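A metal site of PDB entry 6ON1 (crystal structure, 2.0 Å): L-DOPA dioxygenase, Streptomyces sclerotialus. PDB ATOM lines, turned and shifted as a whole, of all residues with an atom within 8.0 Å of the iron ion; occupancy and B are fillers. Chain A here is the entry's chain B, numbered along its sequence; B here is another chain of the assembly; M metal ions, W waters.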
ATOM      1  N   GLN A  96     -31.030 -10.258  16.395  1.00  0.00           N
ATOM      2  CA  GLN A  96     -30.097  -9.486  15.587  1.00  0.00           C
ATOM      3  C   GLN A  96     -29.079 -10.353  14.869  1.00  0.00           C
ATOM      4  O   GLN A  96     -28.627  -9.995  13.766  1.00  0.00           O
ATOM      5  CB  GLN A  96     -29.372  -8.455  16.475  1.00  0.00           C
ATOM      6  CG  GLN A  96     -28.595  -7.397  15.691  1.00  0.00           C
ATOM      7  CD  GLN A  96     -27.176  -7.839  15.398  1.00  0.00           C
ATOM      8  OE1 GLN A  96     -26.575  -8.557  16.179  1.00  0.00           O
ATOM      9  NE2 GLN A  96     -26.630  -7.414  14.247  1.00  0.00           N
ATOM     10  N   HIS A  97     -28.686 -11.467  15.483  1.00  0.00           N
ATOM     11  CA  HIS A  97     -27.704 -12.338  14.873  1.00  0.00           C
ATOM     12  C   HIS A  97     -27.774 -13.718  15.517  1.00  0.00           C
ATOM     13  O   HIS A  97     -28.269 -13.892  16.628  1.00  0.00           O
ATOM     14  CB  HIS A  97     -26.280 -11.768  14.987  1.00  0.00           C
ATOM     15  CG  HIS A  97     -25.689 -11.853  16.364  1.00  0.00           C
ATOM     16  ND1 HIS A  97     -25.962 -10.920  17.352  1.00  0.00           N
ATOM     17  CD2 HIS A  97     -24.796 -12.716  16.902  1.00  0.00           C
ATOM     18  CE1 HIS A  97     -25.282 -11.223  18.443  1.00  0.00           C
ATOM     19  NE2 HIS A  97     -24.570 -12.314  18.201  1.00  0.00           N
ATOM     20  N   LEU A  98     -27.279 -14.688  14.756  1.00  0.00           N
ATOM     21  CA  LEU A  98     -27.110 -16.068  15.184  1.00  0.00           C
ATOM     22  C   LEU A  98     -25.624 -16.371  15.191  1.00  0.00           C
ATOM     23  O   LEU A  98     -24.916 -15.994  14.249  1.00  0.00           O
ATOM     24  CB  LEU A  98     -27.808 -17.048  14.237  1.00  0.00           C
ATOM     25  CG  LEU A  98     -29.306 -17.205  14.384  1.00  0.00           C
ATOM     26  CD1 LEU A  98     -29.954 -18.217  13.374  1.00  0.00           C
ATOM     27  CD2 LEU A  98     -29.605 -17.582  15.809  1.00  0.00           C
ATOM     28  N   CYS A  99     -25.160 -17.041  16.228  1.00  0.00           N
ATOM     29  CA  CYS A  99     -23.740 -17.347  16.367  1.00  0.00           C
ATOM     30  C   CYS A  99     -23.527 -18.849  16.322  1.00  0.00           C
ATOM     31  O   CYS A  99     -24.109 -19.589  17.113  1.00  0.00           O
ATOM     32  CB  CYS A  99     -23.170 -16.797  17.663  1.00  0.00           C
ATOM     33  SG  CYS A  99     -21.418 -17.214  17.869  1.00  0.00           S
ATOM     34  N   LEU A 100     -22.640 -19.301  15.438  1.00  0.00           N
ATOM     35  CA  LEU A 100     -22.305 -20.714  15.292  1.00  0.00           C
ATOM     36  C   LEU A 100     -20.879 -20.945  15.763  1.00  0.00           C
ATOM     37  O   LEU A 100     -19.978 -20.184  15.388  1.00  0.00           O
ATOM     38  CB  LEU A 100     -22.479 -21.146  13.852  1.00  0.00           C
ATOM     39  CG  LEU A 100     -23.783 -20.651  13.224  1.00  0.00           C
ATOM     40  CD1 LEU A 100     -23.795 -20.981  11.748  1.00  0.00           C
ATOM     41  CD2 LEU A 100     -24.973 -21.288  13.957  1.00  0.00           C
ATOM     42  N   SER A 144     -13.579 -14.455  16.338  1.00  0.00           N
ATOM     43  CA  SER A 144     -14.872 -13.959  15.885  1.00  0.00           C
ATOM     44  C   SER A 144     -14.788 -13.608  14.414  1.00  0.00           C
ATOM     45  O   SER A 144     -13.748 -13.141  13.926  1.00  0.00           O
ATOM     46  CB  SER A 144     -15.313 -12.722  16.671  1.00  0.00           C
ATOM     47  OG  SER A 144     -15.334 -12.990  18.046  1.00  0.00           O
ATOM     48  N   TYR A 146     -17.795 -12.203  11.271  1.00  0.00           N
ATOM     49  CA  TYR A 146     -19.176 -11.862  10.923  1.00  0.00           C
ATOM     50  C   TYR A 146     -19.337 -11.819   9.407  1.00  0.00           C
ATOM     51  O   TYR A 146     -18.509 -11.242   8.688  1.00  0.00           O
ATOM     52  CB  TYR A 146     -19.602 -10.520  11.541  1.00  0.00           C
ATOM     53  CG  TYR A 146     -19.597 -10.514  13.050  1.00  0.00           C
ATOM     54  CD1 TYR A 146     -20.719 -10.902  13.789  1.00  0.00           C
ATOM     55  CD2 TYR A 146     -18.453 -10.115  13.759  1.00  0.00           C
ATOM     56  CE1 TYR A 146     -20.705 -10.895  15.178  1.00  0.00           C
ATOM     57  CE2 TYR A 146     -18.430 -10.098  15.150  1.00  0.00           C
ATOM     58  CZ  TYR A 146     -19.557 -10.496  15.859  1.00  0.00           C
ATOM     59  OH  TYR A 146     -19.542 -10.507  17.234  1.00  0.00           O
ATOM     60  N   GLU A 154     -27.253 -11.215   9.828  1.00  0.00           N
ATOM     61  CA  GLU A 154     -25.917 -11.416  10.354  1.00  0.00           C
ATOM     62  C   GLU A 154     -25.706 -12.803  10.963  1.00  0.00           C
ATOM     63  O   GLU A 154     -26.463 -13.233  11.846  1.00  0.00           O
ATOM     64  CB  GLU A 154     -25.598 -10.357  11.406  1.00  0.00           C
ATOM     65  CG  GLU A 154     -24.178 -10.467  11.912  1.00  0.00           C
ATOM     66  CD  GLU A 154     -23.733  -9.174  12.570  1.00  0.00           C
ATOM     67  OE1 GLU A 154     -23.283  -8.262  11.857  1.00  0.00           O
ATOM     68  OE2 GLU A 154     -23.883  -9.080  13.801  1.00  0.00           O
ATOM     69  N   TYR A 155     -24.636 -13.460  10.528  1.00  0.00           N
ATOM     70  CA  TYR A 155     -24.167 -14.686  11.147  1.00  0.00           C
ATOM     71  C   TYR A 155     -22.785 -14.451  11.741  1.00  0.00           C
ATOM     72  O   TYR A 155     -21.911 -13.885  11.087  1.00  0.00           O
ATOM     73  CB  TYR A 155     -24.118 -15.836  10.132  1.00  0.00           C
ATOM     74  CG  TYR A 155     -25.487 -16.403   9.878  1.00  0.00           C
ATOM     75  CD1 TYR A 155     -26.320 -15.846   8.933  1.00  0.00           C
ATOM     76  CD2 TYR A 155     -25.949 -17.494  10.604  1.00  0.00           C
ATOM     77  CE1 TYR A 155     -27.587 -16.353   8.697  1.00  0.00           C
ATOM     78  CE2 TYR A 155     -27.216 -18.030  10.375  1.00  0.00           C
ATOM     79  CZ  TYR A 155     -28.028 -17.452   9.419  1.00  0.00           C
ATOM     80  OH  TYR A 155     -29.283 -17.972   9.199  1.00  0.00           O
ATOM     81  N   GLU A 156     -22.610 -14.873  12.985  1.00  0.00           N
ATOM     82  CA  GLU A 156     -21.338 -14.805  13.687  1.00  0.00           C
ATOM     83  C   GLU A 156     -20.758 -16.210  13.780  1.00  0.00           C
ATOM     84  O   GLU A 156     -21.443 -17.142  14.208  1.00  0.00           O
ATOM     85  CB  GLU A 156     -21.533 -14.205  15.091  1.00  0.00           C
ATOM     86  CG  GLU A 156     -20.331 -14.228  16.040  1.00  0.00           C
ATOM     87  CD  GLU A 156     -20.706 -13.786  17.461  1.00  0.00           C
ATOM     88  OE1 GLU A 156     -21.898 -13.504  17.729  1.00  0.00           O
ATOM     89  OE2 GLU A 156     -19.814 -13.721  18.325  1.00  0.00           O
ATOM     90  N   PHE A 157     -19.508 -16.361  13.372  1.00  0.00           N
ATOM     91  CA  PHE A 157     -18.780 -17.592  13.642  1.00  0.00           C
ATOM     92  C   PHE A 157     -17.792 -17.332  14.769  1.00  0.00           C
ATOM     93  O   PHE A 157     -17.137 -16.296  14.796  1.00  0.00           O
ATOM     94  CB  PHE A 157     -18.050 -18.081  12.400  1.00  0.00           C
ATOM     95  CG  PHE A 157     -18.968 -18.545  11.307  1.00  0.00           C
ATOM     96  CD1 PHE A 157     -19.413 -19.849  11.274  1.00  0.00           C
ATOM     97  CD2 PHE A 157     -19.383 -17.671  10.316  1.00  0.00           C
ATOM     98  CE1 PHE A 157     -20.283 -20.290  10.247  1.00  0.00           C
ATOM     99  CE2 PHE A 157     -20.231 -18.085   9.300  1.00  0.00           C
ATOM    100  CZ  PHE A 157     -20.677 -19.389   9.267  1.00  0.00           C
ATOM    101  N   THR A 158     -17.723 -18.261  15.712  1.00  0.00           N
ATOM    102  CA  THR A 158     -16.788 -18.146  16.807  1.00  0.00           C
ATOM    103  C   THR A 158     -15.956 -19.412  16.917  1.00  0.00           C
ATOM    104  O   THR A 158     -16.378 -20.491  16.500  1.00  0.00           O
ATOM    105  CB  THR A 158     -17.498 -17.858  18.153  1.00  0.00           C
ATOM    106  OG1 THR A 158     -16.523 -17.495  19.112  1.00  0.00           O
ATOM    107  CG2 THR A 158     -18.260 -19.098  18.645  1.00  0.00           C
ATOM    108  N   HIS B  20     -24.523 -21.569  18.944  1.00  0.00           N
ATOM    109  CA  HIS B  20     -23.939 -21.090  20.192  1.00  0.00           C
ATOM    110  C   HIS B  20     -24.841 -20.100  20.931  1.00  0.00           C
ATOM    111  O   HIS B  20     -25.140 -20.299  22.105  1.00  0.00           O
ATOM    112  CB  HIS B  20     -22.555 -20.468  19.954  1.00  0.00           C
ATOM    113  CG  HIS B  20     -21.834 -20.105  21.212  1.00  0.00           C
ATOM    114  ND1 HIS B  20     -21.915 -18.851  21.783  1.00  0.00           N
ATOM    115  CD2 HIS B  20     -21.052 -20.835  22.040  1.00  0.00           C
ATOM    116  CE1 HIS B  20     -21.208 -18.826  22.894  1.00  0.00           C
ATOM    117  NE2 HIS B  20     -20.668 -20.014  23.074  1.00  0.00           N
ATOM    118  N   HIS B  21     -25.257 -19.018  20.285  1.00  0.00           N
ATOM    119  CA  HIS B  21     -26.139 -18.070  20.942  1.00  0.00           C
ATOM    120  C   HIS B  21     -26.925 -17.312  19.890  1.00  0.00           C
ATOM    121  O   HIS B  21     -26.557 -17.282  18.714  1.00  0.00           O
ATOM    122  CB  HIS B  21     -25.352 -17.098  21.869  1.00  0.00           C
ATOM    123  CG  HIS B  21     -24.417 -16.171  21.134  1.00  0.00           C
ATOM    124  ND1 HIS B  21     -23.060 -16.413  21.039  1.00  0.00           N
ATOM    125  CD2 HIS B  21     -24.634 -14.974  20.531  1.00  0.00           C
ATOM    126  CE1 HIS B  21     -22.477 -15.410  20.400  1.00  0.00           C
ATOM    127  NE2 HIS B  21     -23.416 -14.530  20.061  1.00  0.00           N
ATOM    128  N   ILE B  22     -28.011 -16.718  20.337  1.00  0.00           N
ATOM    129  CA  ILE B  22     -28.793 -15.779  19.545  1.00  0.00           C
ATOM    130  C   ILE B  22     -28.688 -14.416  20.208  1.00  0.00           C
ATOM    131  O   ILE B  22     -28.702 -14.305  21.434  1.00  0.00           O
ATOM    132  CB  ILE B  22     -30.268 -16.224  19.430  1.00  0.00           C
ATOM    133  CG1 ILE B  22     -31.060 -15.231  18.580  1.00  0.00           C
ATOM    134  CG2 ILE B  22     -30.906 -16.367  20.824  1.00  0.00           C
ATOM    135  CD1 ILE B  22     -32.132 -15.866  17.746  1.00  0.00           C
ATOM    136  N   GLY B  23     -28.581 -13.366  19.390  1.00  0.00           N
ATOM    137  CA  GLY B  23     -28.494 -12.010  19.898  1.00  0.00           C
ATOM    138  C   GLY B  23     -29.861 -11.358  19.870  1.00  0.00           C
ATOM    139  O   GLY B  23     -30.578 -11.448  18.872  1.00  0.00           O
ATOM    140  N   VAL B  24     -30.216 -10.727  20.972  1.00  0.00           N
ATOM    141  CA  VAL B  24     -31.472 -10.007  21.108  1.00  0.00           C
ATOM    142  C   VAL B  24     -31.149  -8.544  21.328  1.00  0.00           C
ATOM    143  O   VAL B  24     -30.605  -8.179  22.389  1.00  0.00           O
ATOM    144  CB  VAL B  24     -32.342 -10.542  22.265  1.00  0.00           C
ATOM    145  CG1 VAL B  24     -33.533  -9.643  22.456  1.00  0.00           C
ATOM    146  CG2 VAL B  24     -32.788 -11.963  21.965  1.00  0.00           C
ATOM    147  N   TRP B  46     -22.508 -13.511  32.476  1.00  0.00           N
ATOM    148  CA  TRP B  46     -21.574 -12.385  32.503  1.00  0.00           C
ATOM    149  C   TRP B  46     -22.260 -11.197  31.859  1.00  0.00           C
ATOM    150  O   TRP B  46     -23.300 -11.328  31.205  1.00  0.00           O
ATOM    151  CB  TRP B  46     -20.240 -12.683  31.801  1.00  0.00           C
ATOM    152  CG  TRP B  46     -20.329 -13.315  30.411  1.00  0.00           C
ATOM    153  CD1 TRP B  46     -20.183 -14.656  30.102  1.00  0.00           C
ATOM    154  CD2 TRP B  46     -20.502 -12.632  29.153  1.00  0.00           C
ATOM    155  NE1 TRP B  46     -20.288 -14.841  28.732  1.00  0.00           N
ATOM    156  CE2 TRP B  46     -20.487 -13.622  28.133  1.00  0.00           C
ATOM    157  CE3 TRP B  46     -20.712 -11.301  28.789  1.00  0.00           C
ATOM    158  CZ2 TRP B  46     -20.653 -13.320  26.775  1.00  0.00           C
ATOM    159  CZ3 TRP B  46     -20.866 -10.989  27.419  1.00  0.00           C
ATOM    160  CH2 TRP B  46     -20.839 -12.004  26.436  1.00  0.00           C
ATOM    161  N   THR B  55     -16.822  -5.505  17.507  1.00  0.00           N
ATOM    162  CA  THR B  55     -18.158  -5.494  18.086  1.00  0.00           C
ATOM    163  C   THR B  55     -18.828  -4.142  17.862  1.00  0.00           C
ATOM    164  O   THR B  55     -19.990  -4.075  17.431  1.00  0.00           O
ATOM    165  CB  THR B  55     -18.093  -5.807  19.584  1.00  0.00           C
ATOM    166  OG1 THR B  55     -17.703  -7.167  19.765  1.00  0.00           O
ATOM    167  CG2 THR B  55     -19.439  -5.586  20.191  1.00  0.00           C
ATOM    168  N   LEU B  59     -22.342  -3.323  15.912  1.00  0.00           N
ATOM    169  CA  LEU B  59     -23.405  -2.802  16.772  1.00  0.00           C
ATOM    170  C   LEU B  59     -23.027  -1.396  17.239  1.00  0.00           C
ATOM    171  O   LEU B  59     -22.732  -1.184  18.421  1.00  0.00           O
ATOM    172  CB  LEU B  59     -23.643  -3.743  17.955  1.00  0.00           C
ATOM    173  CG  LEU B  59     -23.985  -5.195  17.595  1.00  0.00           C
ATOM    174  CD1 LEU B  59     -23.924  -6.049  18.875  1.00  0.00           C
ATOM    175  CD2 LEU B  59     -25.350  -5.268  16.947  1.00  0.00           C
ATOM    176  N   LEU B  65     -23.877  -5.460  27.247  1.00  0.00           N
ATOM    177  CA  LEU B  65     -24.193  -6.766  26.698  1.00  0.00           C
ATOM    178  C   LEU B  65     -24.204  -7.778  27.835  1.00  0.00           C
ATOM    179  O   LEU B  65     -23.314  -7.765  28.685  1.00  0.00           O
ATOM    180  CB  LEU B  65     -23.158  -7.175  25.633  1.00  0.00           C
ATOM    181  CG  LEU B  65     -23.091  -8.641  25.238  1.00  0.00           C
ATOM    182  CD1 LEU B  65     -24.196  -8.950  24.220  1.00  0.00           C
ATOM    183  CD2 LEU B  65     -21.726  -8.973  24.648  1.00  0.00           C
ATOM    184  N   GLU B  67     -24.850 -12.033  28.720  1.00  0.00           N
ATOM    185  CA  GLU B  67     -25.110 -13.393  28.274  1.00  0.00           C
ATOM    186  C   GLU B  67     -26.036 -14.053  29.284  1.00  0.00           C
ATOM    187  O   GLU B  67     -25.682 -14.177  30.453  1.00  0.00           O
ATOM    188  CB  GLU B  67     -23.855 -14.240  28.123  1.00  0.00           C
ATOM    189  CG  GLU B  67     -24.242 -15.718  27.812  1.00  0.00           C
ATOM    190  CD  GLU B  67     -23.075 -16.593  27.422  1.00  0.00           C
ATOM    191  OE1 GLU B  67     -22.541 -16.422  26.297  1.00  0.00           O
ATOM    192  OE2 GLU B  67     -22.690 -17.443  28.243  1.00  0.00           O
ATOM    193  N   HIS B  76     -27.744 -13.579  24.115  1.00  0.00           N
ATOM    194  CA  HIS B  76     -26.993 -12.347  24.340  1.00  0.00           C
ATOM    195  C   HIS B  76     -27.956 -11.184  24.163  1.00  0.00           C
ATOM    196  O   HIS B  76     -28.419 -10.912  23.054  1.00  0.00           O
ATOM    197  CB  HIS B  76     -25.824 -12.231  23.357  1.00  0.00           C
ATOM    198  CG  HIS B  76     -24.691 -13.139  23.673  1.00  0.00           C
ATOM    199  ND1 HIS B  76     -23.424 -12.971  23.154  1.00  0.00           N
ATOM    200  CD2 HIS B  76     -24.624 -14.216  24.501  1.00  0.00           C
ATOM    201  CE1 HIS B  76     -22.631 -13.916  23.624  1.00  0.00           C
ATOM    202  NE2 HIS B  76     -23.336 -14.685  24.436  1.00  0.00           N
ATOM    203  N   PHE B  78     -28.552  -7.162  24.385  1.00  0.00           N
ATOM    204  CA  PHE B  78     -27.775  -5.928  24.391  1.00  0.00           C
ATOM    205  C   PHE B  78     -28.642  -4.741  24.016  1.00  0.00           C
ATOM    206  O   PHE B  78     -29.698  -4.871  23.381  1.00  0.00           O
ATOM    207  CB  PHE B  78     -26.555  -6.009  23.446  1.00  0.00           C
ATOM    208  CG  PHE B  78     -26.910  -6.367  22.031  1.00  0.00           C
ATOM    209  CD1 PHE B  78     -26.992  -7.697  21.631  1.00  0.00           C
ATOM    210  CD2 PHE B  78     -27.149  -5.371  21.100  1.00  0.00           C
ATOM    211  CE1 PHE B  78     -27.319  -8.031  20.329  1.00  0.00           C
ATOM    212  CE2 PHE B  78     -27.476  -5.692  19.776  1.00  0.00           C
ATOM    213  CZ  PHE B  78     -27.561  -7.023  19.390  1.00  0.00           C
HETATM  214 FE    FE M   1     -22.810 -12.634  19.299  1.00  0.00          FE
HETATM  215  O   HOH W   1     -21.995 -10.586  18.704  1.00  0.00           O
HETATM  216  O   HOH W   2     -20.870 -12.687  20.459  1.00  0.00           O
HETATM  217  O   HOH W   3     -23.565 -11.553  20.941  1.00  0.00           O
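ND1 of His 21 of chain B sits at hydrogen-bond distance from ND1 of His 20 of chain B, 2.8 Å away.
The side-chain sulfur of Cys 99 lies close to the backbone carbonyl oxygen of Glu 156 (3.7 Å).
ND1 of His 97 is in hydrogen-bond range of OE1 of Gln 96 (2.7 Å).
A ring nitrogen (NE2) of His 76 of chain B sits at hydrogen-bond distance from the side-chain carboxylate (OE1) of Glu 67 of chain B, at 2.7 Å.
The backbone NH (N) of Gly 23 of chain B sits at hydrogen-bond distance from the backbone carbonyl oxygen (O) of His 97 (2.8 Å).
The side-chain carboxylate (OE2) of Glu 156 is in hydrogen-bond range of the side-chain hydroxyl (OH) of Tyr 146.
O of Leu 98 sits at hydrogen-bond distance from N of Glu 156, 2.9 Å away.
A ring nitrogen (ND1) of His 76 of chain B sits close to a ring nitrogen (NE2) of His 21 of chain B.
ND1 of His 76 of chain B touches the iron ion, at 3.9 Å.
Four residues have an atom within 4 Å of the iron ion: His 97, Glu 156, His 21 of chain B and His 76 of chain B.
OE1 of Glu 156 is bound to the iron ion (2.0 Å).
A ring nitrogen (NE2) of His 97 is bound to the iron ion.
Water W3 binds the iron ion.
The iron ion is bound by NE2 of His 21 of chain B, 2.1 Å away.
The iron ion is bound by water W2 (2.3 Å).
Water W1 binds the iron ion, at 2.3 Å.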
